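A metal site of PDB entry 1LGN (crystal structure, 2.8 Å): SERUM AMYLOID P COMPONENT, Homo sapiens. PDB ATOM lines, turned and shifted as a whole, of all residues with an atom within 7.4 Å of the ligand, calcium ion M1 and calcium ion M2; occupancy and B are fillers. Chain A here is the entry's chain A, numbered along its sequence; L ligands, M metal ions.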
ATOM      1  N   ALA A  46      16.613  15.157  -7.115  1.00  0.00           N
ATOM      2  CA  ALA A  46      17.419  14.120  -7.734  1.00  0.00           C
ATOM      3  C   ALA A  46      17.106  12.837  -7.010  1.00  0.00           C
ATOM      4  O   ALA A  46      16.701  12.843  -5.843  1.00  0.00           O
ATOM      5  CB  ALA A  46      18.877  14.440  -7.605  1.00  0.00           C
ATOM      6  N   SER A  51      20.821   1.305  -8.333  1.00  0.00           N
ATOM      7  CA  SER A  51      22.098   1.293  -7.619  1.00  0.00           C
ATOM      8  C   SER A  51      22.740  -0.087  -7.664  1.00  0.00           C
ATOM      9  O   SER A  51      22.069  -1.091  -7.474  1.00  0.00           O
ATOM     10  CB  SER A  51      21.888   1.741  -6.165  1.00  0.00           C
ATOM     11  OG  SER A  51      23.115   2.078  -5.533  1.00  0.00           O
ATOM     12  N   ASN A  53      26.404  -1.725  -6.182  1.00  0.00           N
ATOM     13  CA  ASN A  53      27.662  -1.609  -5.458  1.00  0.00           C
ATOM     14  C   ASN A  53      28.271  -2.976  -5.195  1.00  0.00           C
ATOM     15  O   ASN A  53      27.554  -3.959  -5.043  1.00  0.00           O
ATOM     16  CB  ASN A  53      27.456  -0.952  -4.091  1.00  0.00           C
ATOM     17  CG  ASN A  53      27.386   0.536  -4.175  1.00  0.00           C
ATOM     18  OD1 ASN A  53      27.120   1.108  -5.228  1.00  0.00           O
ATOM     19  ND2 ASN A  53      27.634   1.187  -3.035  1.00  0.00           N
ATOM     20  N   ASP A  58      31.976   2.084  -4.027  1.00  0.00           N
ATOM     21  CA  ASP A  58      30.716   2.806  -4.072  1.00  0.00           C
ATOM     22  C   ASP A  58      30.456   3.269  -5.508  1.00  0.00           C
ATOM     23  O   ASP A  58      31.377   3.579  -6.232  1.00  0.00           O
ATOM     24  CB  ASP A  58      30.778   4.016  -3.138  1.00  0.00           C
ATOM     25  CG  ASP A  58      29.462   4.793  -3.054  1.00  0.00           C
ATOM     26  OD1 ASP A  58      28.381   4.212  -3.293  1.00  0.00           O
ATOM     27  OD2 ASP A  58      29.487   5.992  -2.722  1.00  0.00           O
ATOM     28  N   ASN A  59      29.191   3.308  -5.901  1.00  0.00           N
ATOM     29  CA  ASN A  59      28.817   3.723  -7.249  1.00  0.00           C
ATOM     30  C   ASN A  59      29.638   2.958  -8.276  1.00  0.00           C
ATOM     31  O   ASN A  59      30.393   3.544  -9.040  1.00  0.00           O
ATOM     32  CB  ASN A  59      29.028   5.225  -7.436  1.00  0.00           C
ATOM     33  CG  ASN A  59      28.354   6.069  -6.362  1.00  0.00           C
ATOM     34  OD1 ASN A  59      27.378   5.649  -5.733  1.00  0.00           O
ATOM     35  ND2 ASN A  59      28.889   7.256  -6.126  1.00  0.00           N
ATOM     36  N   GLU A  60      29.535   1.629  -8.249  1.00  0.00           N
ATOM     37  CA  GLU A  60      30.266   0.825  -9.210  1.00  0.00           C
ATOM     38  C   GLU A  60      29.508   0.923 -10.524  1.00  0.00           C
ATOM     39  O   GLU A  60      30.103   0.983 -11.585  1.00  0.00           O
ATOM     40  CB  GLU A  60      30.396  -0.619  -8.724  1.00  0.00           C
ATOM     41  CG  GLU A  60      31.227  -1.514  -9.634  1.00  0.00           C
ATOM     42  CD  GLU A  60      32.686  -1.097  -9.724  1.00  0.00           C
ATOM     43  OE1 GLU A  60      33.123  -0.247  -8.937  1.00  0.00           O
ATOM     44  OE2 GLU A  60      33.394  -1.634 -10.586  1.00  0.00           O
ATOM     45  N   LEU A  62      25.811   3.015 -11.329  1.00  0.00           N
ATOM     46  CA  LEU A  62      24.659   3.798 -10.826  1.00  0.00           C
ATOM     47  C   LEU A  62      23.995   4.629 -11.919  1.00  0.00           C
ATOM     48  O   LEU A  62      24.669   5.354 -12.636  1.00  0.00           O
ATOM     49  CB  LEU A  62      25.138   4.740  -9.708  1.00  0.00           C
ATOM     50  CG  LEU A  62      24.323   5.943  -9.256  1.00  0.00           C
ATOM     51  CD1 LEU A  62      23.031   5.500  -8.689  1.00  0.00           C
ATOM     52  CD2 LEU A  62      25.093   6.731  -8.197  1.00  0.00           C
ATOM     53  N   TYR A  64      21.711   7.536 -12.165  1.00  0.00           N
ATOM     54  CA  TYR A  64      21.192   8.603 -11.321  1.00  0.00           C
ATOM     55  C   TYR A  64      20.522   9.710 -12.110  1.00  0.00           C
ATOM     56  O   TYR A  64      21.001  10.055 -13.185  1.00  0.00           O
ATOM     57  CB  TYR A  64      22.365   9.189 -10.562  1.00  0.00           C
ATOM     58  CG  TYR A  64      22.050  10.031  -9.373  1.00  0.00           C
ATOM     59  CD1 TYR A  64      21.576   9.467  -8.187  1.00  0.00           C
ATOM     60  CD2 TYR A  64      22.326  11.380  -9.382  1.00  0.00           C
ATOM     61  CE1 TYR A  64      21.390  10.235  -7.041  1.00  0.00           C
ATOM     62  CE2 TYR A  64      22.136  12.154  -8.248  1.00  0.00           C
ATOM     63  CZ  TYR A  64      21.677  11.575  -7.083  1.00  0.00           C
ATOM     64  OH  TYR A  64      21.545  12.344  -5.966  1.00  0.00           O
ATOM     65  N   GLU A  66      19.775  13.544 -12.175  1.00  0.00           N
ATOM     66  CA  GLU A  66      20.155  14.853 -11.649  1.00  0.00           C
ATOM     67  C   GLU A  66      19.014  15.844 -11.459  1.00  0.00           C
ATOM     68  O   GLU A  66      18.921  16.522 -10.439  1.00  0.00           O
ATOM     69  CB  GLU A  66      21.156  15.474 -12.615  1.00  0.00           C
ATOM     70  CG  GLU A  66      22.390  14.623 -12.835  1.00  0.00           C
ATOM     71  CD  GLU A  66      23.235  14.501 -11.583  1.00  0.00           C
ATOM     72  OE1 GLU A  66      23.106  15.370 -10.676  1.00  0.00           O
ATOM     73  OE2 GLU A  66      24.040  13.544 -11.504  1.00  0.00           O
ATOM     74  N   TYR A  74      27.211   6.313 -13.753  1.00  0.00           N
ATOM     75  CA  TYR A  74      28.474   6.175 -13.050  1.00  0.00           C
ATOM     76  C   TYR A  74      29.035   4.781 -13.334  1.00  0.00           C
ATOM     77  O   TYR A  74      28.291   3.798 -13.321  1.00  0.00           O
ATOM     78  CB  TYR A  74      28.267   6.281 -11.558  1.00  0.00           C
ATOM     79  CG  TYR A  74      28.024   7.652 -11.002  1.00  0.00           C
ATOM     80  CD1 TYR A  74      26.822   8.335 -11.228  1.00  0.00           C
ATOM     81  CD2 TYR A  74      28.983   8.269 -10.178  1.00  0.00           C
ATOM     82  CE1 TYR A  74      26.569   9.585 -10.642  1.00  0.00           C
ATOM     83  CE2 TYR A  74      28.740   9.520  -9.595  1.00  0.00           C
ATOM     84  CZ  TYR A  74      27.538  10.167  -9.829  1.00  0.00           C
ATOM     85  OH  TYR A  74      27.291  11.402  -9.261  1.00  0.00           O
ATOM     86  N   LYS A  79      31.721   9.456 -13.842  1.00  0.00           N
ATOM     87  CA  LYS A  79      30.392   9.848 -14.269  1.00  0.00           C
ATOM     88  C   LYS A  79      30.242  10.578 -15.591  1.00  0.00           C
ATOM     89  O   LYS A  79      31.106  11.358 -15.985  1.00  0.00           O
ATOM     90  CB  LYS A  79      29.857  10.726 -13.152  1.00  0.00           C
ATOM     91  CG  LYS A  79      28.621  11.506 -13.419  1.00  0.00           C
ATOM     92  CD  LYS A  79      28.477  12.543 -12.329  1.00  0.00           C
ATOM     93  CE  LYS A  79      27.078  13.126 -12.319  1.00  0.00           C
ATOM     94  NZ  LYS A  79      26.946  14.204 -11.306  1.00  0.00           N
ATOM     95  N   GLN A 135      16.595   3.109  -3.443  1.00  0.00           N
ATOM     96  CA  GLN A 135      17.510   3.796  -2.544  1.00  0.00           C
ATOM     97  C   GLN A 135      18.873   3.895  -3.216  1.00  0.00           C
ATOM     98  O   GLN A 135      19.105   3.262  -4.252  1.00  0.00           O
ATOM     99  CB  GLN A 135      17.667   3.028  -1.243  1.00  0.00           C
ATOM    100  CG  GLN A 135      16.447   3.015  -0.381  1.00  0.00           C
ATOM    101  CD  GLN A 135      16.071   4.384   0.094  1.00  0.00           C
ATOM    102  OE1 GLN A 135      16.906   5.301   0.113  1.00  0.00           O
ATOM    103  NE2 GLN A 135      14.814   4.537   0.461  1.00  0.00           N
ATOM    104  N   GLU A 136      19.752   4.714  -2.664  1.00  0.00           N
ATOM    105  CA  GLU A 136      21.081   4.849  -3.239  1.00  0.00           C
ATOM    106  C   GLU A 136      22.068   4.396  -2.187  1.00  0.00           C
ATOM    107  O   GLU A 136      22.177   4.992  -1.094  1.00  0.00           O
ATOM    108  CB  GLU A 136      21.334   6.301  -3.688  1.00  0.00           C
ATOM    109  CG  GLU A 136      22.465   6.479  -4.704  1.00  0.00           C
ATOM    110  CD  GLU A 136      23.862   6.417  -4.084  1.00  0.00           C
ATOM    111  OE1 GLU A 136      24.106   7.075  -3.047  1.00  0.00           O
ATOM    112  OE2 GLU A 136      24.731   5.715  -4.646  1.00  0.00           O
ATOM    113  N   GLN A 137      22.750   3.309  -2.501  1.00  0.00           N
ATOM    114  CA  GLN A 137      23.717   2.734  -1.572  1.00  0.00           C
ATOM    115  C   GLN A 137      24.968   3.570  -1.478  1.00  0.00           C
ATOM    116  O   GLN A 137      25.413   4.142  -2.467  1.00  0.00           O
ATOM    117  CB  GLN A 137      24.143   1.348  -2.032  1.00  0.00           C
ATOM    118  CG  GLN A 137      23.074   0.306  -2.085  1.00  0.00           C
ATOM    119  CD  GLN A 137      23.530  -0.906  -2.873  1.00  0.00           C
ATOM    120  OE1 GLN A 137      24.410  -1.644  -2.424  1.00  0.00           O
ATOM    121  NE2 GLN A 137      22.950  -1.115  -4.059  1.00  0.00           N
ATOM    122  N   ASP A 138      25.520   3.646  -0.285  1.00  0.00           N
ATOM    123  CA  ASP A 138      26.778   4.337  -0.055  1.00  0.00           C
ATOM    124  C   ASP A 138      27.706   3.342   0.620  1.00  0.00           C
ATOM    125  O   ASP A 138      28.814   3.662   1.025  1.00  0.00           O
ATOM    126  CB  ASP A 138      26.611   5.595   0.783  1.00  0.00           C
ATOM    127  CG  ASP A 138      26.194   6.796  -0.044  1.00  0.00           C
ATOM    128  OD1 ASP A 138      26.230   6.695  -1.294  1.00  0.00           O
ATOM    129  OD2 ASP A 138      25.842   7.840   0.568  1.00  0.00           O
ATOM    130  N   SER A 139      27.225   2.107   0.712  1.00  0.00           N
ATOM    131  CA  SER A 139      27.950   0.991   1.286  1.00  0.00           C
ATOM    132  C   SER A 139      27.449  -0.255   0.547  1.00  0.00           C
ATOM    133  O   SER A 139      26.603  -0.160  -0.346  1.00  0.00           O
ATOM    134  CB  SER A 139      27.692   0.885   2.790  1.00  0.00           C
ATOM    135  OG  SER A 139      26.373   0.468   3.074  1.00  0.00           O
ATOM    136  N   GLY A 142      23.912  -0.955   1.772  1.00  0.00           N
ATOM    137  CA  GLY A 142      23.356  -0.069   2.769  1.00  0.00           C
ATOM    138  C   GLY A 142      23.704   1.413   2.694  1.00  0.00           C
ATOM    139  O   GLY A 142      23.986   1.954   1.622  1.00  0.00           O
ATOM    140  N   LYS A 143      23.663   2.056   3.859  1.00  0.00           N
ATOM    141  CA  LYS A 143      23.918   3.484   4.025  1.00  0.00           C
ATOM    142  C   LYS A 143      23.127   4.332   3.032  1.00  0.00           C
ATOM    143  O   LYS A 143      23.690   5.050   2.205  1.00  0.00           O
ATOM    144  CB  LYS A 143      25.413   3.794   3.979  1.00  0.00           C
ATOM    145  N   PHE A 144      21.805   4.244   3.147  1.00  0.00           N
ATOM    146  CA  PHE A 144      20.864   4.961   2.298  1.00  0.00           C
ATOM    147  C   PHE A 144      20.710   6.429   2.675  1.00  0.00           C
ATOM    148  O   PHE A 144      20.735   6.780   3.860  1.00  0.00           O
ATOM    149  CB  PHE A 144      19.503   4.273   2.357  1.00  0.00           C
ATOM    150  CG  PHE A 144      19.526   2.853   1.889  1.00  0.00           C
ATOM    151  CD1 PHE A 144      20.526   2.403   1.037  1.00  0.00           C
ATOM    152  CD2 PHE A 144      18.547   1.967   2.294  1.00  0.00           C
ATOM    153  CE1 PHE A 144      20.536   1.097   0.592  1.00  0.00           C
ATOM    154  CE2 PHE A 144      18.557   0.661   1.850  1.00  0.00           C
ATOM    155  CZ  PHE A 144      19.546   0.219   0.998  1.00  0.00           C
ATOM    156  N   ASP A 145      20.564   7.271   1.644  1.00  0.00           N
ATOM    157  CA  ASP A 145      20.340   8.693   1.836  1.00  0.00           C
ATOM    158  C   ASP A 145      18.991   9.095   1.230  1.00  0.00           C
ATOM    159  O   ASP A 145      18.829   8.999  -0.007  1.00  0.00           O
ATOM    160  CB  ASP A 145      21.509   9.516   1.286  1.00  0.00           C
ATOM    161  CG  ASP A 145      21.608  10.873   1.968  1.00  0.00           C
ATOM    162  OD1 ASP A 145      20.618  11.640   1.889  1.00  0.00           O
ATOM    163  OD2 ASP A 145      22.657  11.173   2.568  1.00  0.00           O
ATOM    164  N   ARG A 146      18.139   9.496   2.192  1.00  0.00           N
ATOM    165  CA  ARG A 146      16.731   9.876   2.029  1.00  0.00           C
ATOM    166  C   ARG A 146      16.506  10.849   0.923  1.00  0.00           C
ATOM    167  O   ARG A 146      15.497  10.748   0.218  1.00  0.00           O
ATOM    168  CB  ARG A 146      16.144  10.493   3.326  1.00  0.00           C
ATOM    169  CG  ARG A 146      14.718  11.014   3.145  1.00  0.00           C
ATOM    170  CD  ARG A 146      14.259  11.876   4.325  1.00  0.00           C
ATOM    171  NE  ARG A 146      13.400  11.137   5.240  1.00  0.00           N
ATOM    172  CZ  ARG A 146      12.087  10.967   5.082  1.00  0.00           C
ATOM    173  NH1 ARG A 146      11.457  11.475   4.033  1.00  0.00           N
ATOM    174  NH2 ARG A 146      11.393  10.274   5.996  1.00  0.00           N
ATOM    175  N   SER A 147      17.411  11.778   0.781  1.00  0.00           N
ATOM    176  CA  SER A 147      17.286  12.778  -0.243  1.00  0.00           C
ATOM    177  C   SER A 147      17.610  12.235  -1.636  1.00  0.00           C
ATOM    178  O   SER A 147      17.587  12.970  -2.617  1.00  0.00           O
ATOM    179  CB  SER A 147      18.161  13.998   0.066  1.00  0.00           C
ATOM    180  OG  SER A 147      19.468  13.600   0.458  1.00  0.00           O
ATOM    181  N   GLN A 148      17.916  10.948  -1.707  1.00  0.00           N
ATOM    182  CA  GLN A 148      18.205  10.309  -2.982  1.00  0.00           C
ATOM    183  C   GLN A 148      17.231   9.182  -3.244  1.00  0.00           C
ATOM    184  O   GLN A 148      17.285   8.569  -4.300  1.00  0.00           O
ATOM    185  CB  GLN A 148      19.640   9.777  -3.024  1.00  0.00           C
ATOM    186  CG  GLN A 148      20.651  10.883  -3.001  1.00  0.00           C
ATOM    187  CD  GLN A 148      22.056  10.382  -3.092  1.00  0.00           C
ATOM    188  OE1 GLN A 148      22.461   9.499  -2.336  1.00  0.00           O
ATOM    189  NE2 GLN A 148      22.827  10.966  -3.995  1.00  0.00           N
HETATM  190  O1  LIG L   1      26.858  10.593  -4.661  1.00  0.00           O
HETATM  191  C1  LIG L   1      25.992  10.545  -5.769  1.00  0.00           C
HETATM  192  C2  LIG L   1      25.677  11.989  -6.176  1.00  0.00           C
HETATM  193  O2  LIG L   1      24.639  12.543  -5.344  1.00  0.00           O
HETATM  194  C3  LIG L   1      26.883  12.883  -5.980  1.00  0.00           C
HETATM  195  O3  LIG L   1      26.843  13.880  -6.972  1.00  0.00           O
HETATM  196  C4  LIG L   1      26.655  13.580  -4.668  1.00  0.00           C
HETATM  197  C5  LIG L   1      25.154  13.654  -4.598  1.00  0.00           C
HETATM  198  N1  LIG L   1      24.708  13.473  -3.229  1.00  0.00           N
HETATM  199  C6  LIG L   1      25.054  12.533  -2.320  1.00  0.00           C
HETATM  200  N2  LIG L   1      24.466  12.625  -1.167  1.00  0.00           N
HETATM  201  C7  LIG L   1      23.657  13.720  -1.312  1.00  0.00           C
HETATM  202  C8  LIG L   1      22.751  14.359  -0.443  1.00  0.00           C
HETATM  203  N3  LIG L   1      22.493  13.945   0.795  1.00  0.00           N
HETATM  204  N4  LIG L   1      22.099  15.466  -0.900  1.00  0.00           N
HETATM  205  C9  LIG L   1      22.354  15.876  -2.147  1.00  0.00           C
HETATM  206  N5  LIG L   1      23.179  15.330  -3.074  1.00  0.00           N
HETATM  207  C10 LIG L   1      23.800  14.252  -2.575  1.00  0.00           C
HETATM  208  P1  LIG L   1      26.861   9.533  -3.485  1.00  0.00           P
HETATM  209  O4  LIG L   1      27.961  10.020  -2.595  1.00  0.00           O
HETATM  210  O5  LIG L   1      25.540   9.552  -2.751  1.00  0.00           O
HETATM  211  O6  LIG L   1      27.136   8.194  -4.154  1.00  0.00           O
HETATM  212 CA    CA M   1      26.725   6.042  -3.515  1.00  0.00          CA
HETATM  213 CA    CA M   2      24.249   8.451  -1.060  1.00  0.00          CA
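N3 of the ligand is in hydrogen-bond range of OG of Ser 147 (3.1 Å). OD1 of Asp 145 lies within hydrogen-bond range of N3 of the ligand (3.2 Å). The side-chain hydroxyl (OH) of Tyr 64 sits at hydrogen-bond distance from an oxygen (O2) of the ligand (3.2 Å). The side-chain hydroxyl (OH) of Tyr 74 sits at hydrogen-bond distance from an oxygen (O3) of the ligand, 3.4 Å away.
The side-chain amide nitrogen of Gln 148 lies within hydrogen-bond range of the side-chain hydroxyl of Tyr 64, at 2.7 Å. OH of Tyr 74 sits close to NZ of Lys 79 (3.5 Å). N of Tyr 74 lies within hydrogen-bond range of O of Leu 62 (2.9 Å). The side-chain amide oxygen (OE1) of Gln 137 lies close to the backbone carbonyl oxygen (O) of Ser 139 (3.4 Å). The side-chain amide nitrogen of Asn 53 lies close to the side-chain carboxylate of Asp 58, 3.1 Å away. The side-chain amide oxygen (OD1) of Asn 53 is in hydrogen-bond range of the backbone NH (N) of Asn 59, 3.1 Å away. The side-chain hydroxyl (OG) of Ser 51 sits at hydrogen-bond distance from the backbone NH (N) of Gln 137 (3.3 Å). The backbone NH (N) of Asp 138 sits close to the backbone carbonyl oxygen (O) of Lys 143, 3.4 Å away.
Hydrophobic or aromatic side chains that line the ligand: Tyr 64. Nine residues have an atom within 4 Å of the ligand: Asp 58, Asn 59, Tyr 64, Tyr 74, Glu 136, Asp 138, Asp 145, Ser 147 and Gln 148. Along chain A the residues within 4 Å of the ligand span positions 58 to 148.
Within 4 Å of calcium ion M1: Asp 58, Asn 59, Glu 136, Gln 137 and Asp 138. Along chain A the residues within 4 Å of calcium ion M1 span positions 58 to 138. The nearest printed residue that does not touch calcium ion M1 is Asn 53 (5.0 Å).
Merely in contact with calcium ion M2: Asp 145 (3.8 Å). Within 4 Å of calcium ion M2: Glu 136, Asp 138, Asp 145 and Gln 148. The nearest printed residue that does not touch calcium ion M2 is Gln 137 (4.7 Å).
Calcium ion M1 is bound by O6 of the ligand, OE2 of Glu 136, OD1 of Asn 59, OD1 of Asp 138, OD1 of Asp 58, O of Gln 137, OE1 of Glu 136 and OD2 of Asp 58.
Calcium ion M2 is bound by OD2 of Asp 138 (2.4 Å), O5 of the ligand (2.4 Å), OE1 of Glu 136 (2.4 Å), OE1 of Gln 148 (2.4 Å) and OD1 of Asp 138 (2.7 Å). Calcium ion M2 has five donor atoms within binding distance.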
